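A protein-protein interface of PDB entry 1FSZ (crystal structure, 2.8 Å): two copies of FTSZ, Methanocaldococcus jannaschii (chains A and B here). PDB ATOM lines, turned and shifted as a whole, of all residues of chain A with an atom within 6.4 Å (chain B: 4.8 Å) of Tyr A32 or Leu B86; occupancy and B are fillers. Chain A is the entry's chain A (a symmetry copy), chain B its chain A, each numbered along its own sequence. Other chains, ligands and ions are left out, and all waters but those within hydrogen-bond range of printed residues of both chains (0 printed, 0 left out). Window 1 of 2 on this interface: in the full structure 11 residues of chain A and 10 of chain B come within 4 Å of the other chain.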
ATOM      1  N   LYS A  27     -17.201 -19.320  21.946  1.00  0.00           N
ATOM      2  CA  LYS A  27     -16.207 -19.373  20.895  1.00  0.00           C
ATOM      3  C   LYS A  27     -15.038 -20.193  21.410  1.00  0.00           C
ATOM      4  O   LYS A  27     -14.568 -21.108  20.742  1.00  0.00           O
ATOM      5  CB  LYS A  27     -15.726 -17.961  20.540  1.00  0.00           C
ATOM      6  CG  LYS A  27     -16.156 -17.490  19.154  1.00  0.00           C
ATOM      7  CD  LYS A  27     -15.339 -18.174  18.027  1.00  0.00           C
ATOM      8  CE  LYS A  27     -15.758 -19.658  17.754  1.00  0.00           C
ATOM      9  NZ  LYS A  27     -14.592 -20.639  17.623  1.00  0.00           N
ATOM     10  N   GLU A  28     -14.581 -19.848  22.609  1.00  0.00           N
ATOM     11  CA  GLU A  28     -13.454 -20.524  23.261  1.00  0.00           C
ATOM     12  C   GLU A  28     -13.708 -22.017  23.424  1.00  0.00           C
ATOM     13  O   GLU A  28     -12.808 -22.841  23.210  1.00  0.00           O
ATOM     14  CB  GLU A  28     -13.219 -19.919  24.643  1.00  0.00           C
ATOM     15  CG  GLU A  28     -11.774 -19.671  24.995  1.00  0.00           C
ATOM     16  CD  GLU A  28     -11.601 -19.227  26.443  1.00  0.00           C
ATOM     17  OE1 GLU A  28     -12.590 -18.742  27.052  1.00  0.00           O
ATOM     18  OE2 GLU A  28     -10.472 -19.369  26.968  1.00  0.00           O
ATOM     19  N   LEU A  29     -14.934 -22.345  23.840  1.00  0.00           N
ATOM     20  CA  LEU A  29     -15.374 -23.725  24.057  1.00  0.00           C
ATOM     21  C   LEU A  29     -15.278 -24.475  22.730  1.00  0.00           C
ATOM     22  O   LEU A  29     -14.678 -25.567  22.657  1.00  0.00           O
ATOM     23  CB  LEU A  29     -16.818 -23.728  24.576  1.00  0.00           C
ATOM     24  CG  LEU A  29     -17.140 -24.267  25.985  1.00  0.00           C
ATOM     25  CD1 LEU A  29     -15.880 -24.540  26.808  1.00  0.00           C
ATOM     26  CD2 LEU A  29     -18.039 -23.257  26.668  1.00  0.00           C
ATOM     27  N   LEU A  30     -15.866 -23.862  21.694  1.00  0.00           N
ATOM     28  CA  LEU A  30     -15.856 -24.382  20.319  1.00  0.00           C
ATOM     29  C   LEU A  30     -14.408 -24.707  19.903  1.00  0.00           C
ATOM     30  O   LEU A  30     -14.069 -25.824  19.536  1.00  0.00           O
ATOM     31  CB  LEU A  30     -16.431 -23.329  19.387  1.00  0.00           C
ATOM     32  CG  LEU A  30     -17.920 -23.283  19.025  1.00  0.00           C
ATOM     33  CD1 LEU A  30     -18.611 -24.573  19.308  1.00  0.00           C
ATOM     34  CD2 LEU A  30     -18.557 -22.162  19.781  1.00  0.00           C
ATOM     35  N   GLU A  31     -13.560 -23.700  19.980  1.00  0.00           N
ATOM     36  CA  GLU A  31     -12.161 -23.849  19.658  1.00  0.00           C
ATOM     37  C   GLU A  31     -11.580 -25.044  20.372  1.00  0.00           C
ATOM     38  O   GLU A  31     -10.876 -25.853  19.801  1.00  0.00           O
ATOM     39  CB  GLU A  31     -11.407 -22.603  20.103  1.00  0.00           C
ATOM     40  CG  GLU A  31     -10.853 -21.781  18.956  1.00  0.00           C
ATOM     41  CD  GLU A  31     -10.455 -22.659  17.749  1.00  0.00           C
ATOM     42  OE1 GLU A  31      -9.399 -23.346  17.825  1.00  0.00           O
ATOM     43  OE2 GLU A  31     -11.201 -22.668  16.728  1.00  0.00           O
ATOM     44  N   TYR A  32     -11.876 -25.152  21.649  1.00  0.00           N
ATOM     45  CA  TYR A  32     -11.328 -26.251  22.410  1.00  0.00           C
ATOM     46  C   TYR A  32     -11.518 -27.562  21.699  1.00  0.00           C
ATOM     47  O   TYR A  32     -10.586 -28.339  21.575  1.00  0.00           O
ATOM     48  CB  TYR A  32     -11.967 -26.340  23.798  1.00  0.00           C
ATOM     49  CG  TYR A  32     -11.415 -27.507  24.575  1.00  0.00           C
ATOM     50  CD1 TYR A  32     -10.075 -27.535  24.970  1.00  0.00           C
ATOM     51  CD2 TYR A  32     -12.216 -28.617  24.850  1.00  0.00           C
ATOM     52  CE1 TYR A  32      -9.553 -28.641  25.616  1.00  0.00           C
ATOM     53  CE2 TYR A  32     -11.719 -29.726  25.489  1.00  0.00           C
ATOM     54  CZ  TYR A  32     -10.390 -29.752  25.870  1.00  0.00           C
ATOM     55  OH  TYR A  32      -9.890 -30.906  26.471  1.00  0.00           O
ATOM     56  N   LEU A  33     -12.737 -27.798  21.231  1.00  0.00           N
ATOM     57  CA  LEU A  33     -13.074 -29.039  20.568  1.00  0.00           C
ATOM     58  C   LEU A  33     -12.245 -29.285  19.338  1.00  0.00           C
ATOM     59  O   LEU A  33     -12.124 -30.416  18.879  1.00  0.00           O
ATOM     60  CB  LEU A  33     -14.564 -29.045  20.210  1.00  0.00           C
ATOM     61  CG  LEU A  33     -15.467 -29.237  21.441  1.00  0.00           C
ATOM     62  CD1 LEU A  33     -16.888 -29.000  21.074  1.00  0.00           C
ATOM     63  CD2 LEU A  33     -15.315 -30.635  21.996  1.00  0.00           C
ATOM     64  N   GLN A  34     -11.656 -28.228  18.809  1.00  0.00           N
ATOM     65  CA  GLN A  34     -10.871 -28.352  17.600  1.00  0.00           C
ATOM     66  C   GLN A  34      -9.419 -28.708  17.815  1.00  0.00           C
ATOM     67  O   GLN A  34      -8.705 -29.015  16.863  1.00  0.00           O
ATOM     68  CB  GLN A  34     -10.970 -27.067  16.797  1.00  0.00           C
ATOM     69  CG  GLN A  34     -12.342 -26.848  16.204  1.00  0.00           C
ATOM     70  CD  GLN A  34     -12.743 -27.968  15.290  1.00  0.00           C
ATOM     71  OE1 GLN A  34     -11.919 -28.489  14.542  1.00  0.00           O
ATOM     72  NE2 GLN A  34     -14.010 -28.357  15.344  1.00  0.00           N
ATOM     73  N   GLN A  35      -8.965 -28.667  19.056  1.00  0.00           N
ATOM     74  CA  GLN A  35      -7.577 -29.011  19.318  1.00  0.00           C
ATOM     75  C   GLN A  35      -7.375 -30.364  18.680  1.00  0.00           C
ATOM     76  O   GLN A  35      -8.226 -31.242  18.774  1.00  0.00           O
ATOM     77  CB  GLN A  35      -7.307 -29.102  20.816  1.00  0.00           C
ATOM     78  CG  GLN A  35      -6.164 -28.246  21.322  1.00  0.00           C
ATOM     79  CD  GLN A  35      -6.168 -28.144  22.835  1.00  0.00           C
ATOM     80  OE1 GLN A  35      -6.668 -27.154  23.402  1.00  0.00           O
ATOM     81  NE2 GLN A  35      -5.615 -29.170  23.505  1.00  0.00           N
ATOM     82  N   THR A  36      -6.245 -30.538  18.022  1.00  0.00           N
ATOM     83  CA  THR A  36      -5.985 -31.793  17.354  1.00  0.00           C
ATOM     84  C   THR A  36      -4.753 -32.452  17.934  1.00  0.00           C
ATOM     85  O   THR A  36      -4.562 -33.658  17.808  1.00  0.00           O
ATOM     86  CB  THR A  36      -5.765 -31.544  15.864  1.00  0.00           C
ATOM     87  OG1 THR A  36      -5.055 -32.653  15.299  1.00  0.00           O
ATOM     88  CG2 THR A  36      -4.961 -30.244  15.662  1.00  0.00           C
ATOM     89  N   LYS A  39      -1.101 -31.748  24.364  1.00  0.00           N
ATOM     90  CA  LYS A  39      -0.146 -30.776  24.864  1.00  0.00           C
ATOM     91  C   LYS A  39       0.877 -31.477  25.752  1.00  0.00           C
ATOM     92  O   LYS A  39       0.528 -31.919  26.847  1.00  0.00           O
ATOM     93  CB  LYS A  39      -0.882 -29.719  25.664  1.00  0.00           C
ATOM     94  CG  LYS A  39      -1.825 -28.855  24.846  1.00  0.00           C
ATOM     95  CD  LYS A  39      -1.670 -27.392  25.269  1.00  0.00           C
ATOM     96  CE  LYS A  39      -2.808 -26.477  24.781  1.00  0.00           C
ATOM     97  NZ  LYS A  39      -3.981 -26.431  25.721  1.00  0.00           N
ATOM     98  N   ASP A 123      -1.305 -32.009  28.742  1.00  0.00           N
ATOM     99  CA  ASP A 123      -2.152 -33.191  28.672  1.00  0.00           C
ATOM    100  C   ASP A 123      -1.252 -34.328  29.093  1.00  0.00           C
ATOM    101  O   ASP A 123      -1.709 -35.337  29.623  1.00  0.00           O
ATOM    102  CB  ASP A 123      -2.621 -33.418  27.242  1.00  0.00           C
ATOM    103  CG  ASP A 123      -3.889 -32.624  26.899  1.00  0.00           C
ATOM    104  OD1 ASP A 123      -4.997 -32.995  27.384  1.00  0.00           O
ATOM    105  OD2 ASP A 123      -3.779 -31.630  26.134  1.00  0.00           O
ATOM    106  N   ASN B  70     -19.964 -28.546  33.263  1.00  0.00           N
ATOM    107  CA  ASN B  70     -20.258 -29.794  32.588  1.00  0.00           C
ATOM    108  C   ASN B  70     -18.987 -30.402  32.057  1.00  0.00           C
ATOM    109  O   ASN B  70     -18.000 -29.713  31.807  1.00  0.00           O
ATOM    110  CB  ASN B  70     -21.199 -29.555  31.428  1.00  0.00           C
ATOM    111  CG  ASN B  70     -22.040 -30.761  31.117  1.00  0.00           C
ATOM    112  OD1 ASN B  70     -23.230 -30.635  30.860  1.00  0.00           O
ATOM    113  ND2 ASN B  70     -21.431 -31.943  31.141  1.00  0.00           N
ATOM    114  N   THR B  71     -19.017 -31.709  31.885  1.00  0.00           N
ATOM    115  CA  THR B  71     -17.877 -32.463  31.394  1.00  0.00           C
ATOM    116  C   THR B  71     -18.043 -32.684  29.889  1.00  0.00           C
ATOM    117  O   THR B  71     -17.169 -33.221  29.226  1.00  0.00           O
ATOM    118  CB  THR B  71     -17.849 -33.777  32.132  1.00  0.00           C
ATOM    119  OG1 THR B  71     -16.506 -34.180  32.370  1.00  0.00           O
ATOM    120  CG2 THR B  71     -18.595 -34.798  31.365  1.00  0.00           C
ATOM    121  N   ASP B  72     -19.190 -32.227  29.380  1.00  0.00           N
ATOM    122  CA  ASP B  72     -19.615 -32.321  27.980  1.00  0.00           C
ATOM    123  C   ASP B  72     -19.690 -30.915  27.351  1.00  0.00           C
ATOM    124  O   ASP B  72     -20.570 -30.114  27.673  1.00  0.00           O
ATOM    125  CB  ASP B  72     -20.988 -32.997  27.959  1.00  0.00           C
ATOM    126  CG  ASP B  72     -21.592 -33.113  26.562  1.00  0.00           C
ATOM    127  OD1 ASP B  72     -21.830 -32.057  25.932  1.00  0.00           O
ATOM    128  OD2 ASP B  72     -21.847 -34.258  26.103  1.00  0.00           O
ATOM    129  N   ALA B  73     -18.775 -30.619  26.437  1.00  0.00           N
ATOM    130  CA  ALA B  73     -18.728 -29.308  25.811  1.00  0.00           C
ATOM    131  C   ALA B  73     -19.973 -28.909  25.038  1.00  0.00           C
ATOM    132  O   ALA B  73     -20.358 -27.740  25.032  1.00  0.00           O
ATOM    133  CB  ALA B  73     -17.543 -29.238  24.907  1.00  0.00           C
ATOM    134  N   LEU B  76     -22.612 -27.760  27.445  1.00  0.00           N
ATOM    135  CA  LEU B  76     -22.116 -26.549  28.069  1.00  0.00           C
ATOM    136  C   LEU B  76     -22.319 -25.398  27.122  1.00  0.00           C
ATOM    137  O   LEU B  76     -22.789 -24.335  27.506  1.00  0.00           O
ATOM    138  CB  LEU B  76     -20.631 -26.701  28.411  1.00  0.00           C
ATOM    139  CG  LEU B  76     -20.014 -25.623  29.299  1.00  0.00           C
ATOM    140  CD1 LEU B  76     -20.961 -25.316  30.428  1.00  0.00           C
ATOM    141  CD2 LEU B  76     -18.643 -26.091  29.800  1.00  0.00           C
ATOM    142  N   LYS B  84     -19.340 -20.309  32.516  1.00  0.00           N
ATOM    143  CA  LYS B  84     -19.330 -21.709  32.111  1.00  0.00           C
ATOM    144  C   LYS B  84     -17.964 -22.300  32.386  1.00  0.00           C
ATOM    145  O   LYS B  84     -16.935 -21.666  32.157  1.00  0.00           O
ATOM    146  CB  LYS B  84     -19.661 -21.856  30.632  1.00  0.00           C
ATOM    147  CG  LYS B  84     -21.009 -21.236  30.245  1.00  0.00           C
ATOM    148  CD  LYS B  84     -21.117 -21.101  28.745  1.00  0.00           C
ATOM    149  CE  LYS B  84     -22.477 -21.543  28.248  1.00  0.00           C
ATOM    150  NZ  LYS B  84     -22.886 -20.869  26.964  1.00  0.00           N
ATOM    151  N   ILE B  85     -17.943 -23.512  32.904  1.00  0.00           N
ATOM    152  CA  ILE B  85     -16.672 -24.158  33.190  1.00  0.00           C
ATOM    153  C   ILE B  85     -16.679 -25.580  32.608  1.00  0.00           C
ATOM    154  O   ILE B  85     -17.560 -26.380  32.936  1.00  0.00           O
ATOM    155  CB  ILE B  85     -16.427 -24.234  34.718  1.00  0.00           C
ATOM    156  CG1 ILE B  85     -16.537 -22.838  35.319  1.00  0.00           C
ATOM    157  CG2 ILE B  85     -15.062 -24.875  35.011  1.00  0.00           C
ATOM    158  CD1 ILE B  85     -15.896 -22.720  36.665  1.00  0.00           C
ATOM    159  N   LEU B  86     -15.735 -25.895  31.722  1.00  0.00           N
ATOM    160  CA  LEU B  86     -15.685 -27.243  31.167  1.00  0.00           C
ATOM    161  C   LEU B  86     -14.718 -27.975  32.073  1.00  0.00           C
ATOM    162  O   LEU B  86     -13.495 -27.762  32.004  1.00  0.00           O
ATOM    163  CB  LEU B  86     -15.158 -27.227  29.737  1.00  0.00           C
ATOM    164  CG  LEU B  86     -15.109 -28.589  29.044  1.00  0.00           C
ATOM    165  CD1 LEU B  86     -16.524 -29.125  28.848  1.00  0.00           C
ATOM    166  CD2 LEU B  86     -14.403 -28.421  27.705  1.00  0.00           C
ATOM    167  N   ILE B  87     -15.259 -28.820  32.947  1.00  0.00           N
ATOM    168  CA  ILE B  87     -14.403 -29.548  33.883  1.00  0.00           C
ATOM    169  C   ILE B  87     -14.048 -30.885  33.266  1.00  0.00           C
ATOM    170  O   ILE B  87     -14.745 -31.362  32.372  1.00  0.00           O
ATOM    171  CB  ILE B  87     -15.086 -29.753  35.282  1.00  0.00           C
ATOM    172  CG1 ILE B  87     -16.405 -30.469  35.133  1.00  0.00           C
ATOM    173  CG2 ILE B  87     -15.408 -28.418  35.910  1.00  0.00           C
ATOM    174  CD1 ILE B  87     -16.724 -31.267  36.292  1.00  0.00           C
ATOM    175  N   GLY B  88     -12.951 -31.469  33.733  1.00  0.00           N
ATOM    176  CA  GLY B  88     -12.503 -32.748  33.216  1.00  0.00           C
ATOM    177  C   GLY B  88     -11.908 -32.653  31.820  1.00  0.00           C
ATOM    178  O   GLY B  88     -11.986 -33.601  31.037  1.00  0.00           O
ATOM    179  N   LYS B  89     -11.306 -31.514  31.505  1.00  0.00           N
ATOM    180  CA  LYS B  89     -10.710 -31.305  30.199  1.00  0.00           C
ATOM    181  C   LYS B  89      -9.591 -32.292  29.822  1.00  0.00           C
ATOM    182  O   LYS B  89      -9.357 -32.533  28.642  1.00  0.00           O
ATOM    183  CB  LYS B  89     -10.167 -29.889  30.113  1.00  0.00           C
ATOM    184  CG  LYS B  89     -11.130 -28.942  29.521  1.00  0.00           C
ATOM    185  CD  LYS B  89     -10.374 -27.838  28.851  1.00  0.00           C
ATOM    186  CE  LYS B  89     -10.227 -26.656  29.791  1.00  0.00           C
ATOM    187  NZ  LYS B  89     -11.009 -25.472  29.309  1.00  0.00           N
ATOM    188  N   ARG B  93     -12.661 -35.242  27.434  1.00  0.00           N
ATOM    189  CA  ARG B  93     -11.957 -34.343  26.521  1.00  0.00           C
ATOM    190  C   ARG B  93     -12.962 -33.356  26.001  1.00  0.00           C
ATOM    191  O   ARG B  93     -12.834 -32.865  24.904  1.00  0.00           O
ATOM    192  CB  ARG B  93     -11.335 -35.105  25.351  1.00  0.00           C
ATOM    193  CG  ARG B  93      -9.936 -35.679  25.605  1.00  0.00           C
ATOM    194  CD  ARG B  93      -9.366 -36.399  24.355  1.00  0.00           C
ATOM    195  NE  ARG B  93     -10.101 -37.620  23.984  1.00  0.00           N
ATOM    196  CZ  ARG B  93      -9.987 -38.257  22.810  1.00  0.00           C
ATOM    197  NH1 ARG B  93      -9.161 -37.792  21.874  1.00  0.00           N
ATOM    198  NH2 ARG B  93     -10.696 -39.363  22.570  1.00  0.00           N
ATOM    199  N   GLY B  94     -13.980 -33.082  26.802  1.00  0.00           N
ATOM    200  CA  GLY B  94     -15.030 -32.161  26.398  1.00  0.00           C
ATOM    201  C   GLY B  94     -16.126 -32.992  25.770  1.00  0.00           C
ATOM    202  O   GLY B  94     -17.079 -32.499  25.140  1.00  0.00           O
ATOM    203  N   SER B 111     -10.417 -29.940  38.116  1.00  0.00           N
ATOM    204  CA  SER B 111     -10.665 -28.514  37.897  1.00  0.00           C
ATOM    205  C   SER B 111     -11.054 -27.757  39.168  1.00  0.00           C
ATOM    206  O   SER B 111     -11.644 -26.675  39.101  1.00  0.00           O
ATOM    207  CB  SER B 111     -11.772 -28.312  36.862  1.00  0.00           C
ATOM    208  OG  SER B 111     -11.581 -29.107  35.705  1.00  0.00           O
ATOM    209  N   GLU B 114     -10.338 -23.901  39.254  1.00  0.00           N
ATOM    210  CA  GLU B 114     -11.257 -23.160  38.392  1.00  0.00           C
ATOM    211  C   GLU B 114     -12.669 -23.056  38.983  1.00  0.00           C
ATOM    212  O   GLU B 114     -13.291 -21.996  38.921  1.00  0.00           O
ATOM    213  CB  GLU B 114     -11.305 -23.826  37.021  1.00  0.00           C
ATOM    214  CG  GLU B 114     -10.947 -22.914  35.857  1.00  0.00           C
ATOM    215  CD  GLU B 114     -11.600 -23.340  34.514  1.00  0.00           C
ATOM    216  OE1 GLU B 114     -11.407 -24.518  34.091  1.00  0.00           O
ATOM    217  OE2 GLU B 114     -12.296 -22.487  33.885  1.00  0.00           O
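The backbone NH (N) of Ala B73 sits at hydrogen-bond distance from the backbone carbonyl oxygen (O) of Gly B94, 2.8 Å away.
CD2 of Leu B86 touches CD2 of Tyr A32, 3.6 Å away.
Tyr A32 touches Arg B93 (CE2 to O, 3.4 Å).
Leu A33 touches Ala B73 (CD1 to CB, 3.9 Å).
Glu A31 touches none of the printed residues of chain B.
Of chain B, only Leu B86, Lys B89 and Arg B93 come within 4 Å of Tyr A32.
Of the printed residues of chain B, Leu A33 touches Ala B73.
Of chain A, only Tyr A32 comes within 4 Å of Leu B86.
Of the printed residues of chain A, Lys B89 touches Tyr A32 (2.8 Å).
Of the printed residues of chain A, Arg B93 touches Tyr A32.
The nearest residue of chain B that does not touch Tyr A32 is Gly B94 (4.2 Å).
Of the 12 printed residues of chain A, 2 touch a printed residue of chain B.
Among the printed residues, 4 pairs touch across the chains.
The backbone carbonyl oxygen of Lys B89 sits at hydrogen-bond distance from the side-chain hydroxyl of Tyr A32, 2.8 Å away.
No position is printed for both chains.
Of the 4 pairs that touch across the chains among the printed residues, none has its exchanged pair printed and touching as well.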
